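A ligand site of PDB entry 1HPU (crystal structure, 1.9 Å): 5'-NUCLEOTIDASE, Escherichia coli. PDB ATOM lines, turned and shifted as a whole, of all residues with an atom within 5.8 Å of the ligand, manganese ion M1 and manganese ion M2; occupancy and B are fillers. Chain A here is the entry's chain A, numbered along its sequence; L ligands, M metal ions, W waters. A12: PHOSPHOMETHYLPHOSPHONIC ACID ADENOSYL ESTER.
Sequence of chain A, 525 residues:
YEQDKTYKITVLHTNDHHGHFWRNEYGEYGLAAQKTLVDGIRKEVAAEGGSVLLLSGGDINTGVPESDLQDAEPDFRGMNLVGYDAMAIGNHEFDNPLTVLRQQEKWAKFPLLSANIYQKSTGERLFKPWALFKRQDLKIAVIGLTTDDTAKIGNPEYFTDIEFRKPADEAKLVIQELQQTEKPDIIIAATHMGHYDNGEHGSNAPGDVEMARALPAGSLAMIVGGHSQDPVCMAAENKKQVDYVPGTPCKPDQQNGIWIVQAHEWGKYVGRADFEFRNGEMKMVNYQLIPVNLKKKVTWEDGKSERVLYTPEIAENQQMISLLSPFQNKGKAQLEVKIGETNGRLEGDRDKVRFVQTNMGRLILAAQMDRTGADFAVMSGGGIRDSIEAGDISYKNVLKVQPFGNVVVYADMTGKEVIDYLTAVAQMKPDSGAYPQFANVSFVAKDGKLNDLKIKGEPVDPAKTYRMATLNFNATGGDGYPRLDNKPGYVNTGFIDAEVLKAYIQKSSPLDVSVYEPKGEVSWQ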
ATOM      1  N   ASP A  16      11.371   8.291  16.259  1.00  0.00           N
ATOM      2  CA  ASP A  16      12.238   8.278  17.431  1.00  0.00           C
ATOM      3  C   ASP A  16      12.013   7.084  18.365  1.00  0.00           C
ATOM      4  O   ASP A  16      11.931   7.232  19.598  1.00  0.00           O
ATOM      5  CB  ASP A  16      12.056   9.606  18.151  1.00  0.00           C
ATOM      6  CG  ASP A  16      12.593  10.785  17.303  1.00  0.00           C
ATOM      7  OD1 ASP A  16      13.809  11.035  17.395  1.00  0.00           O
ATOM      8  OD2 ASP A  16      11.827  11.394  16.527  1.00  0.00           O
ATOM      9  N   HIS A  18      14.082   4.654  19.012  1.00  0.00           N
ATOM     10  CA  HIS A  18      15.206   4.514  19.932  1.00  0.00           C
ATOM     11  C   HIS A  18      15.344   3.204  20.720  1.00  0.00           C
ATOM     12  O   HIS A  18      15.492   3.234  21.940  1.00  0.00           O
ATOM     13  CB  HIS A  18      15.219   5.690  20.912  1.00  0.00           C
ATOM     14  CG  HIS A  18      15.725   6.969  20.288  1.00  0.00           C
ATOM     15  ND1 HIS A  18      16.910   7.012  19.579  1.00  0.00           N
ATOM     16  CD2 HIS A  18      15.197   8.217  20.234  1.00  0.00           C
ATOM     17  CE1 HIS A  18      17.094   8.244  19.112  1.00  0.00           C
ATOM     18  NE2 HIS A  18      16.076   8.985  19.498  1.00  0.00           N
ATOM     19  N   GLY A  58      12.203   8.113  11.697  1.00  0.00           N
ATOM     20  CA  GLY A  58      13.583   7.782  11.985  1.00  0.00           C
ATOM     21  C   GLY A  58      14.099   7.759  13.410  1.00  0.00           C
ATOM     22  O   GLY A  58      13.374   8.041  14.361  1.00  0.00           O
ATOM     23  N   ASP A  59      15.392   7.494  13.552  1.00  0.00           N
ATOM     24  CA  ASP A  59      16.043   7.382  14.858  1.00  0.00           C
ATOM     25  C   ASP A  59      15.474   6.116  15.542  1.00  0.00           C
ATOM     26  O   ASP A  59      14.907   6.180  16.627  1.00  0.00           O
ATOM     27  CB  ASP A  59      15.799   8.594  15.781  1.00  0.00           C
ATOM     28  CG  ASP A  59      16.979   9.602  15.784  1.00  0.00           C
ATOM     29  OD1 ASP A  59      17.870   9.562  14.901  1.00  0.00           O
ATOM     30  OD2 ASP A  59      17.000  10.457  16.680  1.00  0.00           O
ATOM     31  N   GLY A  90      17.372   8.943  10.400  1.00  0.00           N
ATOM     32  CA  GLY A  90      17.559   9.895  11.482  1.00  0.00           C
ATOM     33  C   GLY A  90      19.050  10.005  11.742  1.00  0.00           C
ATOM     34  O   GLY A  90      19.820   9.238  11.164  1.00  0.00           O
ATOM     35  N   ASN A  91      19.477  10.932  12.597  1.00  0.00           N
ATOM     36  CA  ASN A  91      20.897  11.079  12.850  1.00  0.00           C
ATOM     37  C   ASN A  91      21.467   9.888  13.567  1.00  0.00           C
ATOM     38  O   ASN A  91      22.632   9.511  13.330  1.00  0.00           O
ATOM     39  CB  ASN A  91      21.208  12.364  13.620  1.00  0.00           C
ATOM     40  CG  ASN A  91      20.352  12.534  14.874  1.00  0.00           C
ATOM     41  OD1 ASN A  91      19.142  12.638  14.782  1.00  0.00           O
ATOM     42  ND2 ASN A  91      20.994  12.594  16.027  1.00  0.00           N
ATOM     43  N   HIS A  92      20.669   9.273  14.440  1.00  0.00           N
ATOM     44  CA  HIS A  92      21.152   8.135  15.172  1.00  0.00           C
ATOM     45  C   HIS A  92      21.397   6.880  14.365  1.00  0.00           C
ATOM     46  O   HIS A  92      21.979   5.925  14.886  1.00  0.00           O
ATOM     47  CB  HIS A  92      20.275   7.865  16.401  1.00  0.00           C
ATOM     48  CG  HIS A  92      20.531   8.811  17.519  1.00  0.00           C
ATOM     49  ND1 HIS A  92      21.588   8.666  18.385  1.00  0.00           N
ATOM     50  CD2 HIS A  92      19.948   9.995  17.834  1.00  0.00           C
ATOM     51  CE1 HIS A  92      21.658   9.719  19.181  1.00  0.00           C
ATOM     52  NE2 HIS A  92      20.666  10.541  18.869  1.00  0.00           N
ATOM     53  N   PHE A  94      23.440   6.822  12.303  1.00  0.00           N
ATOM     54  CA  PHE A  94      24.869   6.994  12.026  1.00  0.00           C
ATOM     55  C   PHE A  94      25.651   6.853  13.317  1.00  0.00           C
ATOM     56  O   PHE A  94      26.797   7.307  13.413  1.00  0.00           O
ATOM     57  CB  PHE A  94      25.127   8.377  11.420  1.00  0.00           C
ATOM     58  CG  PHE A  94      24.548   8.530  10.057  1.00  0.00           C
ATOM     59  CD1 PHE A  94      25.193   7.989   8.939  1.00  0.00           C
ATOM     60  CD2 PHE A  94      23.327   9.163   9.870  1.00  0.00           C
ATOM     61  CE1 PHE A  94      24.617   8.069   7.663  1.00  0.00           C
ATOM     62  CE2 PHE A  94      22.740   9.253   8.603  1.00  0.00           C
ATOM     63  CZ  PHE A  94      23.379   8.707   7.509  1.00  0.00           C
ATOM     64  N   ASP A  95      25.037   6.225  14.315  1.00  0.00           N
ATOM     65  CA  ASP A  95      25.726   6.009  15.590  1.00  0.00           C
ATOM     66  C   ASP A  95      26.712   4.843  15.406  1.00  0.00           C
ATOM     67  O   ASP A  95      27.628   4.637  16.201  1.00  0.00           O
ATOM     68  CB  ASP A  95      24.743   5.654  16.713  1.00  0.00           C
ATOM     69  CG  ASP A  95      24.024   6.872  17.291  1.00  0.00           C
ATOM     70  OD1 ASP A  95      24.348   8.016  16.910  1.00  0.00           O
ATOM     71  OD2 ASP A  95      23.128   6.664  18.156  1.00  0.00           O
ATOM     72  N   THR A 147      18.048  15.697   9.178  1.00  0.00           N
ATOM     73  CA  THR A 147      18.586  16.965   9.659  1.00  0.00           C
ATOM     74  C   THR A 147      20.061  17.121   9.317  1.00  0.00           C
ATOM     75  O   THR A 147      20.850  16.189   9.474  1.00  0.00           O
ATOM     76  CB  THR A 147      18.489  17.117  11.176  1.00  0.00           C
ATOM     77  OG1 THR A 147      19.153  18.328  11.556  1.00  0.00           O
ATOM     78  CG2 THR A 147      19.154  15.968  11.899  1.00  0.00           C
ATOM     79  N   ILE A 153      26.450  17.034  15.365  1.00  0.00           N
ATOM     80  CA  ILE A 153      26.203  16.447  16.694  1.00  0.00           C
ATOM     81  C   ILE A 153      26.501  14.955  16.766  1.00  0.00           C
ATOM     82  O   ILE A 153      26.255  14.307  17.786  1.00  0.00           O
ATOM     83  CB  ILE A 153      24.724  16.608  17.107  1.00  0.00           C
ATOM     84  CG1 ILE A 153      23.827  15.821  16.140  1.00  0.00           C
ATOM     85  CG2 ILE A 153      24.353  18.075  17.166  1.00  0.00           C
ATOM     86  CD1 ILE A 153      22.352  15.779  16.500  1.00  0.00           C
ATOM     87  N   GLY A 154      26.995  14.401  15.669  1.00  0.00           N
ATOM     88  CA  GLY A 154      27.323  12.980  15.627  1.00  0.00           C
ATOM     89  C   GLY A 154      28.820  12.782  15.688  1.00  0.00           C
ATOM     90  O   GLY A 154      29.569  13.751  15.799  1.00  0.00           O
ATOM     91  N   ASN A 155      29.263  11.533  15.601  1.00  0.00           N
ATOM     92  CA  ASN A 155      30.684  11.229  15.668  1.00  0.00           C
ATOM     93  C   ASN A 155      31.365  11.555  14.351  1.00  0.00           C
ATOM     94  O   ASN A 155      31.128  10.906  13.358  1.00  0.00           O
ATOM     95  CB  ASN A 155      30.889   9.745  15.995  1.00  0.00           C
ATOM     96  CG  ASN A 155      32.345   9.406  16.258  1.00  0.00           C
ATOM     97  OD1 ASN A 155      32.930   9.828  17.253  1.00  0.00           O
ATOM     98  ND2 ASN A 155      32.942   8.648  15.349  1.00  0.00           N
ATOM     99  N   HIS A 192      13.529  13.779   9.502  1.00  0.00           N
ATOM    100  CA  HIS A 192      14.098  13.726  10.830  1.00  0.00           C
ATOM    101  C   HIS A 192      14.745  15.090  10.990  1.00  0.00           C
ATOM    102  O   HIS A 192      15.973  15.221  10.944  1.00  0.00           O
ATOM    103  CB  HIS A 192      15.151  12.629  10.946  1.00  0.00           C
ATOM    104  CG  HIS A 192      15.489  12.326  12.372  1.00  0.00           C
ATOM    105  ND1 HIS A 192      14.642  11.622  13.193  1.00  0.00           N
ATOM    106  CD2 HIS A 192      16.503  12.775  13.152  1.00  0.00           C
ATOM    107  CE1 HIS A 192      15.107  11.637  14.423  1.00  0.00           C
ATOM    108  NE2 HIS A 192      16.235  12.331  14.436  1.00  0.00           N
ATOM    109  N   ASN A 204      19.564  25.199  16.705  1.00  0.00           N
ATOM    110  CA  ASN A 204      19.365  23.943  15.990  1.00  0.00           C
ATOM    111  C   ASN A 204      19.182  24.216  14.511  1.00  0.00           C
ATOM    112  O   ASN A 204      18.703  25.279  14.119  1.00  0.00           O
ATOM    113  CB  ASN A 204      18.110  23.212  16.484  1.00  0.00           C
ATOM    114  CG  ASN A 204      18.169  22.875  17.962  1.00  0.00           C
ATOM    115  OD1 ASN A 204      18.981  22.054  18.382  1.00  0.00           O
ATOM    116  ND2 ASN A 204      17.308  23.504  18.746  1.00  0.00           N
ATOM    117  N   HIS A 227      12.817  13.688  15.449  1.00  0.00           N
ATOM    118  CA  HIS A 227      14.002  14.346  16.003  1.00  0.00           C
ATOM    119  C   HIS A 227      13.801  15.230  17.250  1.00  0.00           C
ATOM    120  O   HIS A 227      14.497  15.051  18.248  1.00  0.00           O
ATOM    121  CB  HIS A 227      14.669  15.170  14.876  1.00  0.00           C
ATOM    122  CG  HIS A 227      15.998  15.737  15.252  1.00  0.00           C
ATOM    123  ND1 HIS A 227      17.025  14.977  15.754  1.00  0.00           N
ATOM    124  CD2 HIS A 227      16.477  17.010  15.192  1.00  0.00           C
ATOM    125  CE1 HIS A 227      18.073  15.729  15.994  1.00  0.00           C
ATOM    126  NE2 HIS A 227      17.769  16.975  15.654  1.00  0.00           N
ATOM    127  N   GLN A 229      11.376  15.125  19.109  1.00  0.00           N
ATOM    128  CA  GLN A 229      10.630  14.241  19.992  1.00  0.00           C
ATOM    129  C   GLN A 229       9.516  14.942  20.725  1.00  0.00           C
ATOM    130  O   GLN A 229       9.544  15.117  21.942  1.00  0.00           O
ATOM    131  CB  GLN A 229      11.586  13.520  20.958  1.00  0.00           C
ATOM    132  CG  GLN A 229      12.397  12.493  20.164  1.00  0.00           C
ATOM    133  CD  GLN A 229      13.522  11.831  20.968  1.00  0.00           C
ATOM    134  OE1 GLN A 229      14.666  11.742  20.499  1.00  0.00           O
ATOM    135  NE2 GLN A 229      13.214  11.387  22.168  1.00  0.00           N
ATOM    136  N   ARG A 350      18.486  14.656  31.594  1.00  0.00           N
ATOM    137  CA  ARG A 350      18.754  15.681  30.588  1.00  0.00           C
ATOM    138  C   ARG A 350      18.638  17.113  31.103  1.00  0.00           C
ATOM    139  O   ARG A 350      19.495  17.954  30.791  1.00  0.00           O
ATOM    140  CB  ARG A 350      17.811  15.484  29.393  1.00  0.00           C
ATOM    141  CG  ARG A 350      17.917  16.546  28.317  1.00  0.00           C
ATOM    142  CD  ARG A 350      17.232  16.057  27.049  1.00  0.00           C
ATOM    143  NE  ARG A 350      17.160  17.081  26.015  1.00  0.00           N
ATOM    144  CZ  ARG A 350      17.444  16.860  24.736  1.00  0.00           C
ATOM    145  NH1 ARG A 350      17.823  15.645  24.349  1.00  0.00           N
ATOM    146  NH2 ARG A 350      17.330  17.834  23.844  1.00  0.00           N
ATOM    147  N   ARG A 354      22.768  18.832  30.969  1.00  0.00           N
ATOM    148  CA  ARG A 354      22.993  19.774  29.888  1.00  0.00           C
ATOM    149  C   ARG A 354      22.832  21.201  30.412  1.00  0.00           C
ATOM    150  O   ARG A 354      22.806  22.154  29.621  1.00  0.00           O
ATOM    151  CB  ARG A 354      21.988  19.545  28.751  1.00  0.00           C
ATOM    152  CG  ARG A 354      22.029  18.164  28.115  1.00  0.00           C
ATOM    153  CD  ARG A 354      21.295  18.170  26.774  1.00  0.00           C
ATOM    154  NE  ARG A 354      21.258  16.829  26.191  1.00  0.00           N
ATOM    155  CZ  ARG A 354      20.948  16.559  24.925  1.00  0.00           C
ATOM    156  NH1 ARG A 354      20.636  17.547  24.091  1.00  0.00           N
ATOM    157  NH2 ARG A 354      20.941  15.298  24.500  1.00  0.00           N
ATOM    158  N   SER A 380      30.709  15.972  26.761  1.00  0.00           N
ATOM    159  CA  SER A 380      29.444  16.658  26.511  1.00  0.00           C
ATOM    160  C   SER A 380      28.330  16.116  27.419  1.00  0.00           C
ATOM    161  O   SER A 380      28.228  14.902  27.596  1.00  0.00           O
ATOM    162  CB  SER A 380      29.005  16.429  25.068  1.00  0.00           C
ATOM    163  OG  SER A 380      29.893  17.064  24.150  1.00  0.00           O
ATOM    164  N   GLY A 381      27.503  17.002  27.961  1.00  0.00           N
ATOM    165  CA  GLY A 381      26.391  16.571  28.788  1.00  0.00           C
ATOM    166  C   GLY A 381      25.454  15.691  27.961  1.00  0.00           C
ATOM    167  O   GLY A 381      24.771  14.797  28.486  1.00  0.00           O
ATOM    168  N   GLY A 382      25.437  15.944  26.667  1.00  0.00           N
ATOM    169  CA  GLY A 382      24.603  15.166  25.767  1.00  0.00           C
ATOM    170  C   GLY A 382      25.034  13.708  25.687  1.00  0.00           C
ATOM    171  O   GLY A 382      24.286  12.863  25.216  1.00  0.00           O
ATOM    172  N   GLY A 383      26.259  13.430  26.154  1.00  0.00           N
ATOM    173  CA  GLY A 383      26.772  12.066  26.137  1.00  0.00           C
ATOM    174  C   GLY A 383      26.267  11.218  27.308  1.00  0.00           C
ATOM    175  O   GLY A 383      26.485  10.020  27.328  1.00  0.00           O
ATOM    176  N   ARG A 385      23.082   9.842  29.006  1.00  0.00           N
ATOM    177  CA  ARG A 385      21.695   9.603  28.653  1.00  0.00           C
ATOM    178  C   ARG A 385      20.773   8.954  29.688  1.00  0.00           C
ATOM    179  O   ARG A 385      19.649   8.588  29.377  1.00  0.00           O
ATOM    180  CB  ARG A 385      21.667   8.800  27.337  1.00  0.00           C
ATOM    181  CG  ARG A 385      22.186   9.575  26.101  1.00  0.00           C
ATOM    182  CD  ARG A 385      21.442  10.913  25.949  1.00  0.00           C
ATOM    183  NE  ARG A 385      21.760  11.657  24.728  1.00  0.00           N
ATOM    184  CZ  ARG A 385      21.064  11.602  23.609  1.00  0.00           C
ATOM    185  NH1 ARG A 385      19.990  10.823  23.525  1.00  0.00           N
ATOM    186  NH2 ARG A 385      21.408  12.354  22.576  1.00  0.00           N
ATOM    187  N   PHE A 404      26.417   5.145  23.276  1.00  0.00           N
ATOM    188  CA  PHE A 404      26.988   5.382  21.946  1.00  0.00           C
ATOM    189  C   PHE A 404      28.194   4.583  21.537  1.00  0.00           C
ATOM    190  O   PHE A 404      28.591   4.609  20.362  1.00  0.00           O
ATOM    191  CB  PHE A 404      27.268   6.874  21.785  1.00  0.00           C
ATOM    192  CG  PHE A 404      26.084   7.724  22.061  1.00  0.00           C
ATOM    193  CD1 PHE A 404      24.916   7.559  21.316  1.00  0.00           C
ATOM    194  CD2 PHE A 404      26.110   8.670  23.072  1.00  0.00           C
ATOM    195  CE1 PHE A 404      23.789   8.335  21.581  1.00  0.00           C
ATOM    196  CE2 PHE A 404      25.003   9.456  23.349  1.00  0.00           C
ATOM    197  CZ  PHE A 404      23.838   9.297  22.611  1.00  0.00           C
ATOM    198  N   ASN A 406      31.171   5.192  22.408  1.00  0.00           N
ATOM    199  CA  ASN A 406      32.307   6.097  22.192  1.00  0.00           C
ATOM    200  C   ASN A 406      33.542   5.423  22.828  1.00  0.00           C
ATOM    201  O   ASN A 406      33.420   4.524  23.674  1.00  0.00           O
ATOM    202  CB  ASN A 406      32.091   7.459  22.850  1.00  0.00           C
ATOM    203  CG  ASN A 406      31.076   8.331  22.113  1.00  0.00           C
ATOM    204  OD1 ASN A 406      30.731   9.430  22.573  1.00  0.00           O
ATOM    205  ND2 ASN A 406      30.606   7.857  20.972  1.00  0.00           N
ATOM    206  N   SER A 432      21.942  22.520  25.937  1.00  0.00           N
ATOM    207  CA  SER A 432      22.521  22.032  24.693  1.00  0.00           C
ATOM    208  C   SER A 432      23.287  20.744  24.963  1.00  0.00           C
ATOM    209  O   SER A 432      23.877  20.603  26.028  1.00  0.00           O
ATOM    210  CB  SER A 432      23.499  23.037  24.106  1.00  0.00           C
ATOM    211  OG  SER A 432      24.241  22.413  23.073  1.00  0.00           O
ATOM    212  N   GLY A 433      23.294  19.841  23.997  1.00  0.00           N
ATOM    213  CA  GLY A 433      24.026  18.599  24.177  1.00  0.00           C
ATOM    214  C   GLY A 433      25.499  18.881  24.390  1.00  0.00           C
ATOM    215  O   GLY A 433      26.207  18.094  25.029  1.00  0.00           O
ATOM    216  N   ALA A 434      25.951  20.030  23.890  1.00  0.00           N
ATOM    217  CA  ALA A 434      27.357  20.427  24.003  1.00  0.00           C
ATOM    218  C   ALA A 434      27.802  20.996  25.355  1.00  0.00           C
ATOM    219  O   ALA A 434      29.000  21.138  25.577  1.00  0.00           O
ATOM    220  CB  ALA A 434      27.700  21.430  22.882  1.00  0.00           C
ATOM    221  N   PHE A 473      34.541  11.086  20.469  1.00  0.00           N
ATOM    222  CA  PHE A 473      33.495  11.951  19.974  1.00  0.00           C
ATOM    223  C   PHE A 473      33.868  13.439  20.145  1.00  0.00           C
ATOM    224  O   PHE A 473      33.813  14.194  19.195  1.00  0.00           O
ATOM    225  CB  PHE A 473      32.162  11.690  20.699  1.00  0.00           C
ATOM    226  CG  PHE A 473      31.099  12.719  20.373  1.00  0.00           C
ATOM    227  CD1 PHE A 473      30.330  12.610  19.221  1.00  0.00           C
ATOM    228  CD2 PHE A 473      30.905  13.819  21.209  1.00  0.00           C
ATOM    229  CE1 PHE A 473      29.376  13.603  18.899  1.00  0.00           C
ATOM    230  CE2 PHE A 473      29.963  14.798  20.895  1.00  0.00           C
ATOM    231  CZ  PHE A 473      29.197  14.696  19.750  1.00  0.00           C
ATOM    232  N   ASP A 479      30.271  18.017  18.688  1.00  0.00           N
ATOM    233  CA  ASP A 479      29.589  19.095  19.434  1.00  0.00           C
ATOM    234  C   ASP A 479      30.336  20.435  19.324  1.00  0.00           C
ATOM    235  O   ASP A 479      30.133  21.346  20.129  1.00  0.00           O
ATOM    236  CB  ASP A 479      29.408  18.730  20.912  1.00  0.00           C
ATOM    237  CG  ASP A 479      28.093  18.020  21.174  1.00  0.00           C
ATOM    238  OD1 ASP A 479      27.184  18.127  20.326  1.00  0.00           O
ATOM    239  OD2 ASP A 479      27.958  17.353  22.224  1.00  0.00           O
HETATM  240  PB  A12 L   1      19.101  13.684  19.212  1.00  0.00           P
HETATM  241  O1B A12 L   1      18.945  13.256  17.785  1.00  0.00           O
HETATM  242  O2B A12 L   1      17.843  13.430  19.985  1.00  0.00           O
HETATM  243  O3B A12 L   1      20.198  12.938  19.875  1.00  0.00           O
HETATM  244  PA  A12 L   1      19.786  16.020  20.944  1.00  0.00           P
HETATM  245  O1A A12 L   1      18.679  15.618  21.857  1.00  0.00           O
HETATM  246  O2A A12 L   1      19.942  17.493  20.900  1.00  0.00           O
HETATM  247  C3A A12 L   1      19.452  15.414  19.314  1.00  0.00           C
HETATM  248  O5' A12 L   1      21.130  15.349  21.484  1.00  0.00           O
HETATM  249  C5' A12 L   1      22.313  15.545  20.742  1.00  0.00           C
HETATM  250  C4' A12 L   1      23.523  15.429  21.630  1.00  0.00           C
HETATM  251  O4' A12 L   1      23.684  14.048  22.065  1.00  0.00           O
HETATM  252  C3' A12 L   1      24.809  15.773  20.917  1.00  0.00           C
HETATM  253  O3' A12 L   1      24.995  17.182  20.984  1.00  0.00           O
HETATM  254  C2' A12 L   1      25.841  14.983  21.713  1.00  0.00           C
HETATM  255  O2' A12 L   1      26.161  15.618  22.921  1.00  0.00           O
HETATM  256  C1' A12 L   1      25.062  13.693  22.039  1.00  0.00           C
HETATM  257  N9  A12 L   1      25.255  12.628  21.050  1.00  0.00           N
HETATM  258  C8  A12 L   1      24.378  12.244  20.072  1.00  0.00           C
HETATM  259  N7  A12 L   1      24.810  11.254  19.319  1.00  0.00           N
HETATM  260  C5  A12 L   1      26.056  10.966  19.859  1.00  0.00           C
HETATM  261  C6  A12 L   1      27.010   9.997  19.522  1.00  0.00           C
HETATM  262  N6  A12 L   1      26.858   9.113  18.548  1.00  0.00           N
HETATM  263  N1  A12 L   1      28.159   9.972  20.242  1.00  0.00           N
HETATM  264  C2  A12 L   1      28.305  10.850  21.239  1.00  0.00           C
HETATM  265  N3  A12 L   1      27.461  11.797  21.670  1.00  0.00           N
HETATM  266  C4  A12 L   1      26.347  11.805  20.921  1.00  0.00           C
HETATM  267 MN    MN M   1      17.493  12.742  16.241  1.00  0.00          MN
HETATM  268 MN    MN M   2      15.550  10.956  18.502  1.00  0.00          MN
HETATM  269  O   HOH W   1      24.281  11.215  16.277  1.00  0.00           O
HETATM  270  O   HOH W   2      28.611   6.556  18.071  1.00  0.00           O
HETATM  271  O   HOH W   3      16.732  13.105  23.100  1.00  0.00           O
HETATM  272  O   HOH W   4      15.648  15.454  20.700  1.00  0.00           O
HETATM  273  O   HOH W   5      28.425  13.407  23.561  1.00  0.00           O
HETATM  274  O   HOH W   6      16.231  13.012  18.164  1.00  0.00           O
HETATM  275  O   HOH W   7      22.837  19.097  20.962  1.00  0.00           O
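Four residues have an atom within 4 Å of manganese ion M2: Asp 16, His 18, Asp 59 and Gln 229.
The nearest printed residue that does not touch manganese ion M2 is His 192 (4.2 Å).
Water W6 lies within hydrogen-bond range of an oxygen (O2B) of the ligand and the backbone carbonyl oxygen of His 227.
Water W5 lies within hydrogen-bond range of N3 of the ligand (2.7 Å) and N of Gly 383 (3.4 Å).
Water W7 bridges an oxygen (O3') of the ligand (2.9 Å) and the backbone NH (N) of Gly 433 (3.2 Å).
Water W4 lies within hydrogen-bond range of the backbone carbonyl oxygen (O) of His 227 (2.7 Å) and an oxygen (O2B) of the ligand (3.1 Å).
Water W1 bridges a nitrogen (N7) of the ligand and the side-chain carboxylate (OD1) of Asp 95.
Water W3 lies within hydrogen-bond range of NH1 of Arg 350 (3.0 Å) and O2B of the ligand (3.3 Å).
An oxygen (O4') of the ligand lies close to the backbone carbonyl oxygen (O) of Gly 382, at 3.4 Å.
O of Ile 153 touches C8 of the ligand (3.6 Å).
Ser 380 touches the ligand.
Gly 383 touches the ligand (N to O2', 3.9 Å).
CG of Phe 404 touches C6 of the ligand (3.5 Å).
Phe 473 touches the ligand.
Hydrophobic or aromatic side chains within 4 Å of the ligand: His 92, Ile 153, His 227, Phe 404 and Phe 473.
Along chain A the residues within 4 Å of the ligand span positions 59 to 479.
The nearest printed residue that does not touch the ligand is Ala 434 (4.2 Å).
Manganese ion M2 is bound by the side-chain carboxylate (OD1) of Asp 16 (2.1 Å), water W6 (2.2 Å), a ring nitrogen (NE2) of His 18 (2.3 Å), the side-chain amide oxygen (OE1) of Gln 229 (2.3 Å) and the side-chain carboxylate (OD2) of Asp 59 (2.4 Å).
Manganese ion M2 has five donor atoms within binding distance.
Along chain A the residues within 4 Å of manganese ion M1 span positions 59 to 227.
OD2 of Asp 16 lies within hydrogen-bond range of N of His 227, at 2.7 Å.
The backbone carbonyl oxygen of Gly 58 lies within hydrogen-bond range of the backbone NH of Asp 16 (2.8 Å).
The backbone NH of Thr 147 is in hydrogen-bond range of the backbone carbonyl oxygen of His 192 (2.8 Å).
N of His 92 is in hydrogen-bond range of OD1 of Asp 59, 2.9 Å away.
OD2 of Asp 479 sits at hydrogen-bond distance from OG of Ser 380.
The side-chain carboxylate (OD2) of Asp 95 is in hydrogen-bond range of a ring nitrogen (ND1) of His 92.
The guanidinium group (NE) of Arg 385 sits at hydrogen-bond distance from the backbone carbonyl oxygen (O) of Gly 382.
The backbone NH of Gly 382 is in hydrogen-bond range of the backbone carbonyl oxygen of Gly 433 (2.8 Å).
The side-chain carboxylate (OD1) of Asp 479 sits at hydrogen-bond distance from an oxygen (O3') of the ligand (2.5 Å).
An oxygen (O1A) of the ligand lies within salt-bridge range of the guanidinium group (NH1) of Arg 350 (2.6 Å).
NE2 of His 92 lies within hydrogen-bond range of O3B of the ligand, 2.6 Å away.
The guanidinium group (NH2) of Arg 385 lies within salt-bridge range of an oxygen (O3B) of the ligand (3.0 Å).
The guanidinium group of Arg 354 is in salt-bridge range of an oxygen (O2A) of the ligand (3.3 Å).
N1 of the ligand sits at hydrogen-bond distance from ND2 of Asn 406.
OD1 of Asp 95 is in hydrogen-bond range of N6 of the ligand, at 3.2 Å.
O of Gly 433 lies within hydrogen-bond range of O2' of the ligand (3.3 Å).
O1B of the ligand is bound to manganese ion M1 (2.2 Å).
Manganese ion M1 is bound by OD1 of Asn 91, at 2.2 Å.
A ring nitrogen (NE2) of His 192 is bound to manganese ion M1 (2.2 Å).
Water W6 is bound to manganese ion M1 (2.3 Å).
Manganese ion M1 is bound by ND1 of His 227 (2.3 Å).
Manganese ion M1 is bound by OD2 of Asp 59, at 2.4 Å.
Manganese ion M1 has six donor atoms within binding distance.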
